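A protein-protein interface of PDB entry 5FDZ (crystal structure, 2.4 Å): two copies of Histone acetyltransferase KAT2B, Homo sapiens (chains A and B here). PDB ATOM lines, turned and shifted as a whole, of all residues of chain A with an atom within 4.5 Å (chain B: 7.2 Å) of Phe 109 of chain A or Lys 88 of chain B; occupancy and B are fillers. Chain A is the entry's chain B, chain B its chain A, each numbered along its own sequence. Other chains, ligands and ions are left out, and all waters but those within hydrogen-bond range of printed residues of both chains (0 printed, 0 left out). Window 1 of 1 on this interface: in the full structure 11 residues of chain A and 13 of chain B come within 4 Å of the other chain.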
ATOM      1  N   LYS A  88     -15.995 -40.261  20.909  1.00  0.00           N
ATOM      2  CA  LYS A  88     -15.188 -39.458  21.820  1.00  0.00           C
ATOM      3  C   LYS A  88     -15.842 -39.285  23.156  1.00  0.00           C
ATOM      4  O   LYS A  88     -15.179 -39.143  24.185  1.00  0.00           O
ATOM      5  CB  LYS A  88     -14.951 -38.100  21.218  1.00  0.00           C
ATOM      6  CG  LYS A  88     -14.024 -38.123  20.052  1.00  0.00           C
ATOM      7  CD  LYS A  88     -14.082 -36.767  19.423  1.00  0.00           C
ATOM      8  CE  LYS A  88     -12.951 -36.543  18.476  1.00  0.00           C
ATOM      9  NZ  LYS A  88     -13.322 -35.486  17.515  1.00  0.00           N
ATOM     10  N   GLU A 105     -11.715 -38.012  11.313  1.00  0.00           N
ATOM     11  CA  GLU A 105     -12.411 -36.733  11.222  1.00  0.00           C
ATOM     12  C   GLU A 105     -11.617 -35.696  10.439  1.00  0.00           C
ATOM     13  O   GLU A 105     -12.175 -34.994   9.606  1.00  0.00           O
ATOM     14  CB  GLU A 105     -12.701 -36.193  12.606  1.00  0.00           C
ATOM     15  CG  GLU A 105     -13.638 -35.004  12.602  1.00  0.00           C
ATOM     16  CD  GLU A 105     -13.845 -34.449  13.993  1.00  0.00           C
ATOM     17  OE1 GLU A 105     -12.825 -34.226  14.696  1.00  0.00           O
ATOM     18  OE2 GLU A 105     -15.016 -34.214  14.361  1.00  0.00           O
ATOM     19  N   LYS A 106     -10.322 -35.595  10.723  1.00  0.00           N
ATOM     20  CA  LYS A 106      -9.431 -34.717   9.953  1.00  0.00           C
ATOM     21  C   LYS A 106      -9.517 -35.043   8.475  1.00  0.00           C
ATOM     22  O   LYS A 106      -9.637 -34.147   7.651  1.00  0.00           O
ATOM     23  CB  LYS A 106      -7.985 -34.875  10.386  1.00  0.00           C
ATOM     24  CG  LYS A 106      -7.551 -34.046  11.558  1.00  0.00           C
ATOM     25  CD  LYS A 106      -6.078 -34.297  11.753  1.00  0.00           C
ATOM     26  CE  LYS A 106      -5.523 -33.510  12.897  1.00  0.00           C
ATOM     27  NZ  LYS A 106      -4.137 -33.969  13.159  1.00  0.00           N
ATOM     28  N   PHE A 107      -9.457 -36.339   8.156  1.00  0.00           N
ATOM     29  CA  PHE A 107      -9.463 -36.810   6.777  1.00  0.00           C
ATOM     30  C   PHE A 107     -10.770 -36.426   6.126  1.00  0.00           C
ATOM     31  O   PHE A 107     -10.797 -35.846   5.043  1.00  0.00           O
ATOM     32  CB  PHE A 107      -9.260 -38.331   6.734  1.00  0.00           C
ATOM     33  CG  PHE A 107      -9.376 -38.911   5.360  1.00  0.00           C
ATOM     34  CD1 PHE A 107      -8.335 -38.769   4.447  1.00  0.00           C
ATOM     35  CD2 PHE A 107     -10.527 -39.580   4.964  1.00  0.00           C
ATOM     36  CE1 PHE A 107      -8.442 -39.296   3.169  1.00  0.00           C
ATOM     37  CE2 PHE A 107     -10.644 -40.100   3.683  1.00  0.00           C
ATOM     38  CZ  PHE A 107      -9.606 -39.955   2.784  1.00  0.00           C
ATOM     39  N   PHE A 108     -11.847 -36.742   6.820  1.00  0.00           N
ATOM     40  CA  PHE A 108     -13.190 -36.354   6.436  1.00  0.00           C
ATOM     41  C   PHE A 108     -13.331 -34.867   6.075  1.00  0.00           C
ATOM     42  O   PHE A 108     -13.755 -34.547   4.967  1.00  0.00           O
ATOM     43  CB  PHE A 108     -14.114 -36.728   7.568  1.00  0.00           C
ATOM     44  CG  PHE A 108     -15.411 -36.001   7.569  1.00  0.00           C
ATOM     45  CD1 PHE A 108     -16.293 -36.110   6.484  1.00  0.00           C
ATOM     46  CD2 PHE A 108     -15.789 -35.246   8.687  1.00  0.00           C
ATOM     47  CE1 PHE A 108     -17.513 -35.456   6.514  1.00  0.00           C
ATOM     48  CE2 PHE A 108     -17.011 -34.586   8.721  1.00  0.00           C
ATOM     49  CZ  PHE A 108     -17.870 -34.693   7.631  1.00  0.00           C
ATOM     50  N   PHE A 109     -12.939 -33.965   6.977  1.00  0.00           N
ATOM     51  CA  PHE A 109     -13.055 -32.519   6.702  1.00  0.00           C
ATOM     52  C   PHE A 109     -12.250 -32.117   5.487  1.00  0.00           C
ATOM     53  O   PHE A 109     -12.687 -31.259   4.741  1.00  0.00           O
ATOM     54  CB  PHE A 109     -12.623 -31.639   7.902  1.00  0.00           C
ATOM     55  CG  PHE A 109     -13.662 -31.512   8.991  1.00  0.00           C
ATOM     56  CD1 PHE A 109     -14.891 -30.937   8.734  1.00  0.00           C
ATOM     57  CD2 PHE A 109     -13.398 -31.953  10.274  1.00  0.00           C
ATOM     58  CE1 PHE A 109     -15.857 -30.833   9.731  1.00  0.00           C
ATOM     59  CE2 PHE A 109     -14.351 -31.856  11.269  1.00  0.00           C
ATOM     60  CZ  PHE A 109     -15.581 -31.292  10.996  1.00  0.00           C
ATOM     61  N   SER A 110     -11.072 -32.720   5.292  1.00  0.00           N
ATOM     62  CA  SER A 110     -10.242 -32.392   4.133  1.00  0.00           C
ATOM     63  C   SER A 110     -10.937 -32.815   2.834  1.00  0.00           C
ATOM     64  O   SER A 110     -10.839 -32.126   1.831  1.00  0.00           O
ATOM     65  CB  SER A 110      -8.840 -33.022   4.234  1.00  0.00           C
ATOM     66  OG  SER A 110      -8.859 -34.402   3.901  1.00  0.00           O
ATOM     67  N   LYS A 111     -11.658 -33.926   2.868  1.00  0.00           N
ATOM     68  CA  LYS A 111     -12.389 -34.402   1.691  1.00  0.00           C
ATOM     69  C   LYS A 111     -13.646 -33.592   1.366  1.00  0.00           C
ATOM     70  O   LYS A 111     -13.968 -33.428   0.190  1.00  0.00           O
ATOM     71  CB  LYS A 111     -12.740 -35.902   1.823  1.00  0.00           C
ATOM     72  CG  LYS A 111     -11.529 -36.820   1.763  1.00  0.00           C
ATOM     73  CD  LYS A 111     -10.960 -36.896   0.347  1.00  0.00           C
ATOM     74  CE  LYS A 111      -9.452 -37.055   0.347  1.00  0.00           C
ATOM     75  NZ  LYS A 111      -8.926 -37.075  -1.045  1.00  0.00           N
ATOM     76  N   ILE A 112     -14.368 -33.122   2.391  1.00  0.00           N
ATOM     77  CA  ILE A 112     -15.560 -32.273   2.156  1.00  0.00           C
ATOM     78  C   ILE A 112     -15.169 -30.884   1.655  1.00  0.00           C
ATOM     79  O   ILE A 112     -15.825 -30.351   0.764  1.00  0.00           O
ATOM     80  CB  ILE A 112     -16.560 -32.191   3.330  1.00  0.00           C
ATOM     81  CG1 ILE A 112     -16.000 -31.298   4.473  1.00  0.00           C
ATOM     82  CG2 ILE A 112     -17.026 -33.608   3.731  1.00  0.00           C
ATOM     83  CD1 ILE A 112     -16.850 -31.236   5.736  1.00  0.00           C
ATOM     84  N   LYS A 113     -14.082 -30.324   2.192  1.00  0.00           N
ATOM     85  CA  LYS A 113     -13.543 -29.065   1.679  1.00  0.00           C
ATOM     86  C   LYS A 113     -13.077 -29.233   0.230  1.00  0.00           C
ATOM     87  O   LYS A 113     -13.363 -28.379  -0.596  1.00  0.00           O
ATOM     88  CB  LYS A 113     -12.428 -28.494   2.579  1.00  0.00           C
ATOM     89  CG  LYS A 113     -12.937 -27.886   3.895  1.00  0.00           C
ATOM     90  CD  LYS A 113     -11.864 -27.926   4.982  1.00  0.00           C
ATOM     91  CE  LYS A 113     -12.281 -27.228   6.264  1.00  0.00           C
ATOM     92  NZ  LYS A 113     -11.317 -27.483   7.386  1.00  0.00           N
ATOM     93  N   PHE B  36     -11.361 -19.679  21.933  1.00  0.00           N
ATOM     94  CA  PHE B  36     -12.806 -19.907  21.988  1.00  0.00           C
ATOM     95  C   PHE B  36     -13.515 -19.038  23.010  1.00  0.00           C
ATOM     96  O   PHE B  36     -14.715 -19.199  23.263  1.00  0.00           O
ATOM     97  CB  PHE B  36     -13.062 -21.393  22.304  1.00  0.00           C
ATOM     98  CG  PHE B  36     -12.217 -22.344  21.485  1.00  0.00           C
ATOM     99  CD1 PHE B  36     -12.450 -22.515  20.126  1.00  0.00           C
ATOM    100  CD2 PHE B  36     -11.169 -23.068  22.067  1.00  0.00           C
ATOM    101  CE1 PHE B  36     -11.662 -23.378  19.370  1.00  0.00           C
ATOM    102  CE2 PHE B  36     -10.387 -23.929  21.305  1.00  0.00           C
ATOM    103  CZ  PHE B  36     -10.629 -24.076  19.959  1.00  0.00           C
ATOM    104  N   ILE B  52     -20.004 -19.904   8.712  1.00  0.00           N
ATOM    105  CA  ILE B  52     -20.479 -20.432   9.975  1.00  0.00           C
ATOM    106  C   ILE B  52     -21.803 -19.762  10.338  1.00  0.00           C
ATOM    107  O   ILE B  52     -21.819 -18.591  10.695  1.00  0.00           O
ATOM    108  CB  ILE B  52     -19.416 -20.181  11.064  1.00  0.00           C
ATOM    109  CG1 ILE B  52     -18.064 -20.820  10.671  1.00  0.00           C
ATOM    110  CG2 ILE B  52     -19.874 -20.683  12.422  1.00  0.00           C
ATOM    111  CD1 ILE B  52     -18.065 -22.336  10.536  1.00  0.00           C
ATOM    112  N   GLN B  81     -20.028 -28.563  21.681  1.00  0.00           N
ATOM    113  CA  GLN B  81     -19.604 -29.268  20.438  1.00  0.00           C
ATOM    114  C   GLN B  81     -19.632 -28.323  19.270  1.00  0.00           C
ATOM    115  O   GLN B  81     -18.796 -28.402  18.427  1.00  0.00           O
ATOM    116  CB  GLN B  81     -20.437 -30.491  19.999  1.00  0.00           C
ATOM    117  CG  GLN B  81     -20.514 -31.670  20.966  1.00  0.00           C
ATOM    118  CD  GLN B  81     -19.277 -31.805  21.850  1.00  0.00           C
ATOM    119  OE1 GLN B  81     -19.331 -31.508  23.032  1.00  0.00           O
ATOM    120  NE2 GLN B  81     -18.163 -32.258  21.272  1.00  0.00           N
ATOM    121  N   ARG B  82     -20.607 -27.423  19.223  1.00  0.00           N
ATOM    122  CA  ARG B  82     -20.687 -26.422  18.135  1.00  0.00           C
ATOM    123  C   ARG B  82     -19.443 -25.545  18.085  1.00  0.00           C
ATOM    124  O   ARG B  82     -18.968 -25.208  17.005  1.00  0.00           O
ATOM    125  CB  ARG B  82     -21.901 -25.521  18.314  1.00  0.00           C
ATOM    126  CG  ARG B  82     -22.107 -24.402  17.263  1.00  0.00           C
ATOM    127  CD  ARG B  82     -22.442 -24.879  15.864  1.00  0.00           C
ATOM    128  NE  ARG B  82     -23.743 -25.515  15.819  1.00  0.00           N
ATOM    129  CZ  ARG B  82     -24.191 -26.229  14.792  1.00  0.00           C
ATOM    130  NH1 ARG B  82     -23.437 -26.441  13.707  1.00  0.00           N
ATOM    131  NH2 ARG B  82     -25.403 -26.742  14.856  1.00  0.00           N
ATOM    132  N   VAL B  83     -18.916 -25.183  19.261  1.00  0.00           N
ATOM    133  CA  VAL B  83     -17.669 -24.437  19.336  1.00  0.00           C
ATOM    134  C   VAL B  83     -16.599 -25.196  18.554  1.00  0.00           C
ATOM    135  O   VAL B  83     -15.870 -24.606  17.759  1.00  0.00           O
ATOM    136  CB  VAL B  83     -17.198 -24.187  20.803  1.00  0.00           C
ATOM    137  CG1 VAL B  83     -15.806 -23.593  20.845  1.00  0.00           C
ATOM    138  CG2 VAL B  83     -18.165 -23.285  21.550  1.00  0.00           C
ATOM    139  N   PHE B  84     -16.515 -26.504  18.780  1.00  0.00           N
ATOM    140  CA  PHE B  84     -15.443 -27.310  18.202  1.00  0.00           C
ATOM    141  C   PHE B  84     -15.663 -27.549  16.699  1.00  0.00           C
ATOM    142  O   PHE B  84     -14.726 -27.484  15.917  1.00  0.00           O
ATOM    143  CB  PHE B  84     -15.252 -28.627  18.965  1.00  0.00           C
ATOM    144  CG  PHE B  84     -14.987 -28.462  20.465  1.00  0.00           C
ATOM    145  CD1 PHE B  84     -14.091 -27.500  20.948  1.00  0.00           C
ATOM    146  CD2 PHE B  84     -15.623 -29.296  21.398  1.00  0.00           C
ATOM    147  CE1 PHE B  84     -13.854 -27.358  22.323  1.00  0.00           C
ATOM    148  CE2 PHE B  84     -15.394 -29.163  22.764  1.00  0.00           C
ATOM    149  CZ  PHE B  84     -14.502 -28.193  23.227  1.00  0.00           C
ATOM    150  N   THR B  85     -16.908 -27.772  16.298  1.00  0.00           N
ATOM    151  CA  THR B  85     -17.221 -28.108  14.910  1.00  0.00           C
ATOM    152  C   THR B  85     -17.120 -26.879  14.023  1.00  0.00           C
ATOM    153  O   THR B  85     -16.627 -26.975  12.903  1.00  0.00           O
ATOM    154  CB  THR B  85     -18.610 -28.804  14.762  1.00  0.00           C
ATOM    155  OG1 THR B  85     -19.659 -27.946  15.231  1.00  0.00           O
ATOM    156  CG2 THR B  85     -18.633 -30.101  15.559  1.00  0.00           C
ATOM    157  N   ASN B  86     -17.547 -25.721  14.530  1.00  0.00           N
ATOM    158  CA  ASN B  86     -17.269 -24.436  13.855  1.00  0.00           C
ATOM    159  C   ASN B  86     -15.792 -24.278  13.557  1.00  0.00           C
ATOM    160  O   ASN B  86     -15.415 -23.956  12.437  1.00  0.00           O
ATOM    161  CB  ASN B  86     -17.752 -23.252  14.699  1.00  0.00           C
ATOM    162  CG  ASN B  86     -19.264 -23.086  14.670  1.00  0.00           C
ATOM    163  OD1 ASN B  86     -19.969 -23.793  13.942  1.00  0.00           O
ATOM    164  ND2 ASN B  86     -19.773 -22.186  15.500  1.00  0.00           N
ATOM    165  N   CYS B  87     -14.966 -24.522  14.565  1.00  0.00           N
ATOM    166  CA  CYS B  87     -13.517 -24.363  14.442  1.00  0.00           C
ATOM    167  C   CYS B  87     -12.900 -25.311  13.418  1.00  0.00           C
ATOM    168  O   CYS B  87     -12.012 -24.921  12.660  1.00  0.00           O
ATOM    169  CB  CYS B  87     -12.827 -24.544  15.809  1.00  0.00           C
ATOM    170  SG  CYS B  87     -11.027 -24.469  15.734  1.00  0.00           S
ATOM    171  N   LYS B  88     -13.349 -26.555  13.415  1.00  0.00           N
ATOM    172  CA  LYS B  88     -12.773 -27.562  12.539  1.00  0.00           C
ATOM    173  C   LYS B  88     -13.271 -27.412  11.099  1.00  0.00           C
ATOM    174  O   LYS B  88     -12.554 -27.731  10.165  1.00  0.00           O
ATOM    175  CB  LYS B  88     -13.104 -28.933  13.063  1.00  0.00           C
ATOM    176  CG  LYS B  88     -12.409 -29.296  14.369  1.00  0.00           C
ATOM    177  CD  LYS B  88     -12.939 -30.645  14.814  1.00  0.00           C
ATOM    178  CE  LYS B  88     -12.205 -31.175  16.022  1.00  0.00           C
ATOM    179  NZ  LYS B  88     -13.120 -31.951  16.918  1.00  0.00           N
ATOM    180  N   GLU B  89     -14.506 -26.926  10.964  1.00  0.00           N
ATOM    181  CA  GLU B  89     -15.109 -26.524   9.675  1.00  0.00           C
ATOM    182  C   GLU B  89     -14.356 -25.388   8.994  1.00  0.00           C
ATOM    183  O   GLU B  89     -14.140 -25.420   7.775  1.00  0.00           O
ATOM    184  CB  GLU B  89     -16.607 -26.086   9.853  1.00  0.00           C
ATOM    185  CG  GLU B  89     -17.633 -27.166   9.478  1.00  0.00           C
ATOM    186  CD  GLU B  89     -18.954 -27.066  10.246  1.00  0.00           C
ATOM    187  OE1 GLU B  89     -19.624 -26.020  10.140  1.00  0.00           O
ATOM    188  OE2 GLU B  89     -19.347 -28.051  10.924  1.00  0.00           O
ATOM    189  N   TYR B  90     -13.969 -24.387   9.774  1.00  0.00           N
ATOM    190  CA  TYR B  90     -13.369 -23.166   9.238  1.00  0.00           C
ATOM    191  C   TYR B  90     -11.839 -23.267   9.063  1.00  0.00           C
ATOM    192  O   TYR B  90     -11.310 -22.794   8.064  1.00  0.00           O
ATOM    193  CB  TYR B  90     -13.761 -21.965  10.114  1.00  0.00           C
ATOM    194  CG  TYR B  90     -13.271 -20.631   9.596  1.00  0.00           C
ATOM    195  CD1 TYR B  90     -13.929 -19.974   8.575  1.00  0.00           C
ATOM    196  CD2 TYR B  90     -12.143 -20.032  10.136  1.00  0.00           C
ATOM    197  CE1 TYR B  90     -13.463 -18.758   8.088  1.00  0.00           C
ATOM    198  CE2 TYR B  90     -11.670 -18.815   9.663  1.00  0.00           C
ATOM    199  CZ  TYR B  90     -12.329 -18.184   8.639  1.00  0.00           C
ATOM    200  OH  TYR B  90     -11.842 -16.987   8.170  1.00  0.00           O
ATOM    201  N   ASN B  91     -11.137 -23.889  10.007  1.00  0.00           N
ATOM    202  CA  ASN B  91      -9.673 -23.888  10.002  1.00  0.00           C
ATOM    203  C   ASN B  91      -9.019 -25.149   9.400  1.00  0.00           C
ATOM    204  O   ASN B  91      -9.621 -26.229   9.382  1.00  0.00           O
ATOM    205  CB  ASN B  91      -9.145 -23.661  11.428  1.00  0.00           C
ATOM    206  CG  ASN B  91      -9.520 -22.292  11.972  1.00  0.00           C
ATOM    207  OD1 ASN B  91      -8.881 -21.287  11.637  1.00  0.00           O
ATOM    208  ND2 ASN B  91     -10.559 -22.237  12.792  1.00  0.00           N
ATOM    209  N   PRO B  92      -7.766 -25.006   8.902  1.00  0.00           N
ATOM    210  CA  PRO B  92      -6.951 -26.150   8.485  1.00  0.00           C
ATOM    211  C   PRO B  92      -6.656 -27.161   9.603  1.00  0.00           C
ATOM    212  O   PRO B  92      -6.447 -26.755  10.747  1.00  0.00           O
ATOM    213  CB  PRO B  92      -5.645 -25.497   8.006  1.00  0.00           C
ATOM    214  CG  PRO B  92      -6.051 -24.151   7.532  1.00  0.00           C
ATOM    215  CD  PRO B  92      -7.163 -23.727   8.456  1.00  0.00           C
ATOM    216  N   PRO B  93      -6.580 -28.466   9.261  1.00  0.00           N
ATOM    217  CA  PRO B  93      -6.387 -29.534  10.265  1.00  0.00           C
ATOM    218  C   PRO B  93      -5.152 -29.396  11.173  1.00  0.00           C
ATOM    219  O   PRO B  93      -5.210 -29.758  12.368  1.00  0.00           O
ATOM    220  CB  PRO B  93      -6.319 -30.831   9.426  1.00  0.00           C
ATOM    221  CG  PRO B  93      -6.727 -30.479   8.038  1.00  0.00           C
ATOM    222  CD  PRO B  93      -6.708 -28.992   7.878  1.00  0.00           C
ATOM    223  N   TYR B  97      -5.461 -23.529  15.960  1.00  0.00           N
ATOM    224  CA  TYR B  97      -6.839 -23.474  16.438  1.00  0.00           C
ATOM    225  C   TYR B  97      -7.505 -24.859  16.389  1.00  0.00           C
ATOM    226  O   TYR B  97      -8.181 -25.260  17.345  1.00  0.00           O
ATOM    227  CB  TYR B  97      -7.688 -22.460  15.648  1.00  0.00           C
ATOM    228  CG  TYR B  97      -7.162 -21.024  15.647  1.00  0.00           C
ATOM    229  CD1 TYR B  97      -6.703 -20.408  16.817  1.00  0.00           C
ATOM    230  CD2 TYR B  97      -7.132 -20.282  14.478  1.00  0.00           C
ATOM    231  CE1 TYR B  97      -6.224 -19.100  16.810  1.00  0.00           C
ATOM    232  CE2 TYR B  97      -6.658 -18.969  14.462  1.00  0.00           C
ATOM    233  CZ  TYR B  97      -6.208 -18.384  15.631  1.00  0.00           C
ATOM    234  OH  TYR B  97      -5.740 -17.085  15.604  1.00  0.00           O
ATOM    235  N   TYR B  98      -7.287 -25.591  15.295  1.00  0.00           N
ATOM    236  CA  TYR B  98      -7.804 -26.962  15.159  1.00  0.00           C
ATOM    237  C   TYR B  98      -7.222 -27.859  16.268  1.00  0.00           C
ATOM    238  O   TYR B  98      -7.962 -28.560  16.916  1.00  0.00           O
ATOM    239  CB  TYR B  98      -7.487 -27.533  13.756  1.00  0.00           C
ATOM    240  CG  TYR B  98      -8.351 -28.698  13.314  1.00  0.00           C
ATOM    241  CD1 TYR B  98      -8.232 -29.959  13.920  1.00  0.00           C
ATOM    242  CD2 TYR B  98      -9.257 -28.565  12.253  1.00  0.00           C
ATOM    243  CE1 TYR B  98      -9.004 -31.041  13.508  1.00  0.00           C
ATOM    244  CE2 TYR B  98     -10.027 -29.651  11.815  1.00  0.00           C
ATOM    245  CZ  TYR B  98      -9.891 -30.886  12.447  1.00  0.00           C
ATOM    246  OH  TYR B  98     -10.654 -31.950  12.058  1.00  0.00           O
ATOM    247  N   LYS B  99      -5.906 -27.813  16.471  1.00  0.00           N
ATOM    248  CA  LYS B  99      -5.242 -28.584  17.539  1.00  0.00           C
ATOM    249  C   LYS B  99      -5.833 -28.278  18.910  1.00  0.00           C
ATOM    250  O   LYS B  99      -6.163 -29.206  19.659  1.00  0.00           O
ATOM    251  CB  LYS B  99      -3.733 -28.315  17.567  1.00  0.00           C
ATOM    252  CG  LYS B  99      -2.989 -28.938  16.402  1.00  0.00           C
ATOM    253  CD  LYS B  99      -1.490 -28.677  16.461  1.00  0.00           C
ATOM    254  CE  LYS B  99      -1.089 -27.471  15.629  1.00  0.00           C
ATOM    255  NZ  LYS B  99       0.273 -27.609  15.056  1.00  0.00           N
ATOM    256  N   ALA B 101      -8.792 -27.076  19.560  1.00  0.00           N
ATOM    257  CA  ALA B 101     -10.163 -27.618  19.593  1.00  0.00           C
ATOM    258  C   ALA B 101     -10.206 -29.064  20.100  1.00  0.00           C
ATOM    259  O   ALA B 101     -11.045 -29.401  20.914  1.00  0.00           O
ATOM    260  CB  ALA B 101     -10.819 -27.524  18.212  1.00  0.00           C
ATOM    261  N   ASN B 102      -9.288 -29.892  19.617  1.00  0.00           N
ATOM    262  CA  ASN B 102      -9.238 -31.310  19.991  1.00  0.00           C
ATOM    263  C   ASN B 102      -8.645 -31.564  21.373  1.00  0.00           C
ATOM    264  O   ASN B 102      -9.059 -32.501  22.057  1.00  0.00           O
ATOM    265  CB  ASN B 102      -8.442 -32.122  18.955  1.00  0.00           C
ATOM    266  CG  ASN B 102      -9.293 -32.571  17.774  1.00  0.00           C
ATOM    267  OD1 ASN B 102     -10.525 -32.647  17.863  1.00  0.00           O
ATOM    268  ND2 ASN B 102      -8.637 -32.844  16.646  1.00  0.00           N
ATOM    269  N   GLU B 105     -11.446 -30.406  23.628  1.00  0.00           N
ATOM    270  CA  GLU B 105     -12.515 -31.405  23.573  1.00  0.00           C
ATOM    271  C   GLU B 105     -12.207 -32.642  24.427  1.00  0.00           C
ATOM    272  O   GLU B 105     -13.067 -33.126  25.138  1.00  0.00           O
ATOM    273  CB  GLU B 105     -12.770 -31.833  22.135  1.00  0.00           C
ATOM    274  CG  GLU B 105     -14.018 -32.687  21.978  1.00  0.00           C
ATOM    275  CD  GLU B 105     -14.225 -33.147  20.555  1.00  0.00           C
ATOM    276  OE1 GLU B 105     -13.245 -33.656  19.963  1.00  0.00           O
ATOM    277  OE2 GLU B 105     -15.363 -32.973  20.035  1.00  0.00           O
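The side-chain carboxylate (OE1) of Glu 105 of chain A lies within salt-bridge range of the side-chain amino group (NZ) of Lys 88 of chain B (3.2 Å).
O of Lys 88 of chain B is in hydrogen-bond range of NZ of Lys 113 of chain A (3.1 Å).
The backbone carbonyl oxygen of Asn 91 of chain B is in hydrogen-bond range of the side-chain amino group of Lys 113 of chain A.
The side-chain carboxylate (OE1) of Glu 105 of chain B lies within salt-bridge range of the side-chain amino group (NZ) of Lys 88 of chain A (3.1 Å).
The side-chain carboxylate (OE2) of Glu 105 of chain B sits at hydrogen-bond distance from the side-chain amide nitrogen (NE2) of Gln 81 of chain B (3.1 Å).
The side-chain amide nitrogen (ND2) of Asn 91 of chain B sits at hydrogen-bond distance from the backbone carbonyl oxygen (O) of Cys 87 of chain B (3.1 Å).
OD1 of Asn 102 of chain B sits at hydrogen-bond distance from NZ of Lys 88 of chain B (2.8 Å).
The side-chain amino group (NZ) of Lys 88 of chain B lies within salt-bridge range of the side-chain carboxylate (OE1) of Glu 105 of chain B.
The side-chain amino group (NZ) of Lys 88 of chain A lies within salt-bridge range of the side-chain carboxylate (OE1) of Glu 105 of chain A (3.1 Å).
Among the printed residues, merely in contact across the chains: Lys 113 of chain A with Glu 89 of chain B (3.0 Å), Phe 109 of chain A with Tyr 98 of chain B (3.3 Å), Lys 88 of chain A with Lys 88 of chain B (3.6 Å), Phe 109 of chain A with Lys 88 of chain B (3.6 Å), Lys 106 of chain A with Tyr 98 of chain B (3.7 Å) and Lys 106 of chain A with Pro 93 of chain B (3.8 Å).
Printed residues of chain B within 4 Å of Lys 88 of chain A: Lys 88 and Glu 105.
Of chain B, only Lys 88 (3.6 Å) and Tyr 98 (3.3 Å) come within 4 Å of Phe 109 of chain A.
Printed residues of chain B within 4 Å of Lys 113 of chain A: Lys 88 (3.1 Å), Glu 89 (3.0 Å) and Asn 91 (2.9 Å).
Lys 88 of chain B touches just these residues of chain A: Lys 88 (3.6 Å), Glu 105 (3.2 Å), Phe 109 (3.6 Å) and Lys 113 (3.1 Å).
Of the printed residues of chain A, Tyr 98 of chain B touches Lys 106 (3.7 Å) and Phe 109 (3.3 Å).
The nearest residue of chain B that does not touch Phe 109 of chain A is Glu 89 of chain B (4.1 Å).
The nearest printed residue of chain A that does not touch Tyr 98 of chain B is Glu 105 of chain A (4.1 Å).
Hydrophobic or aromatic side chains of chain B within 4 Å of the printed part of chain A: Tyr 98.
Of the 10 printed residues of chain A, 5 touch a printed residue of chain B.
Printed residues of chain A that touch a printed residue of chain B: Lys 88, Glu 105, Lys 106, Phe 109 and Lys 113.
Hydrophobic or aromatic side chains of chain A that line the printed part of chain B: Phe 109.
Among the printed residues, 10 pairs touch across the chains.
Lys 88 of chain B touches its own counterpart, Lys 88 of chain A.
Lys 88 of chain A touches Glu 105 of chain B, and with the chains exchanged Glu 105 of chain A touches Lys 88 of chain B.
Of the 10 pairs that touch across the chains among the printed residues, 3 have their exchanged pair printed and touching as well.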
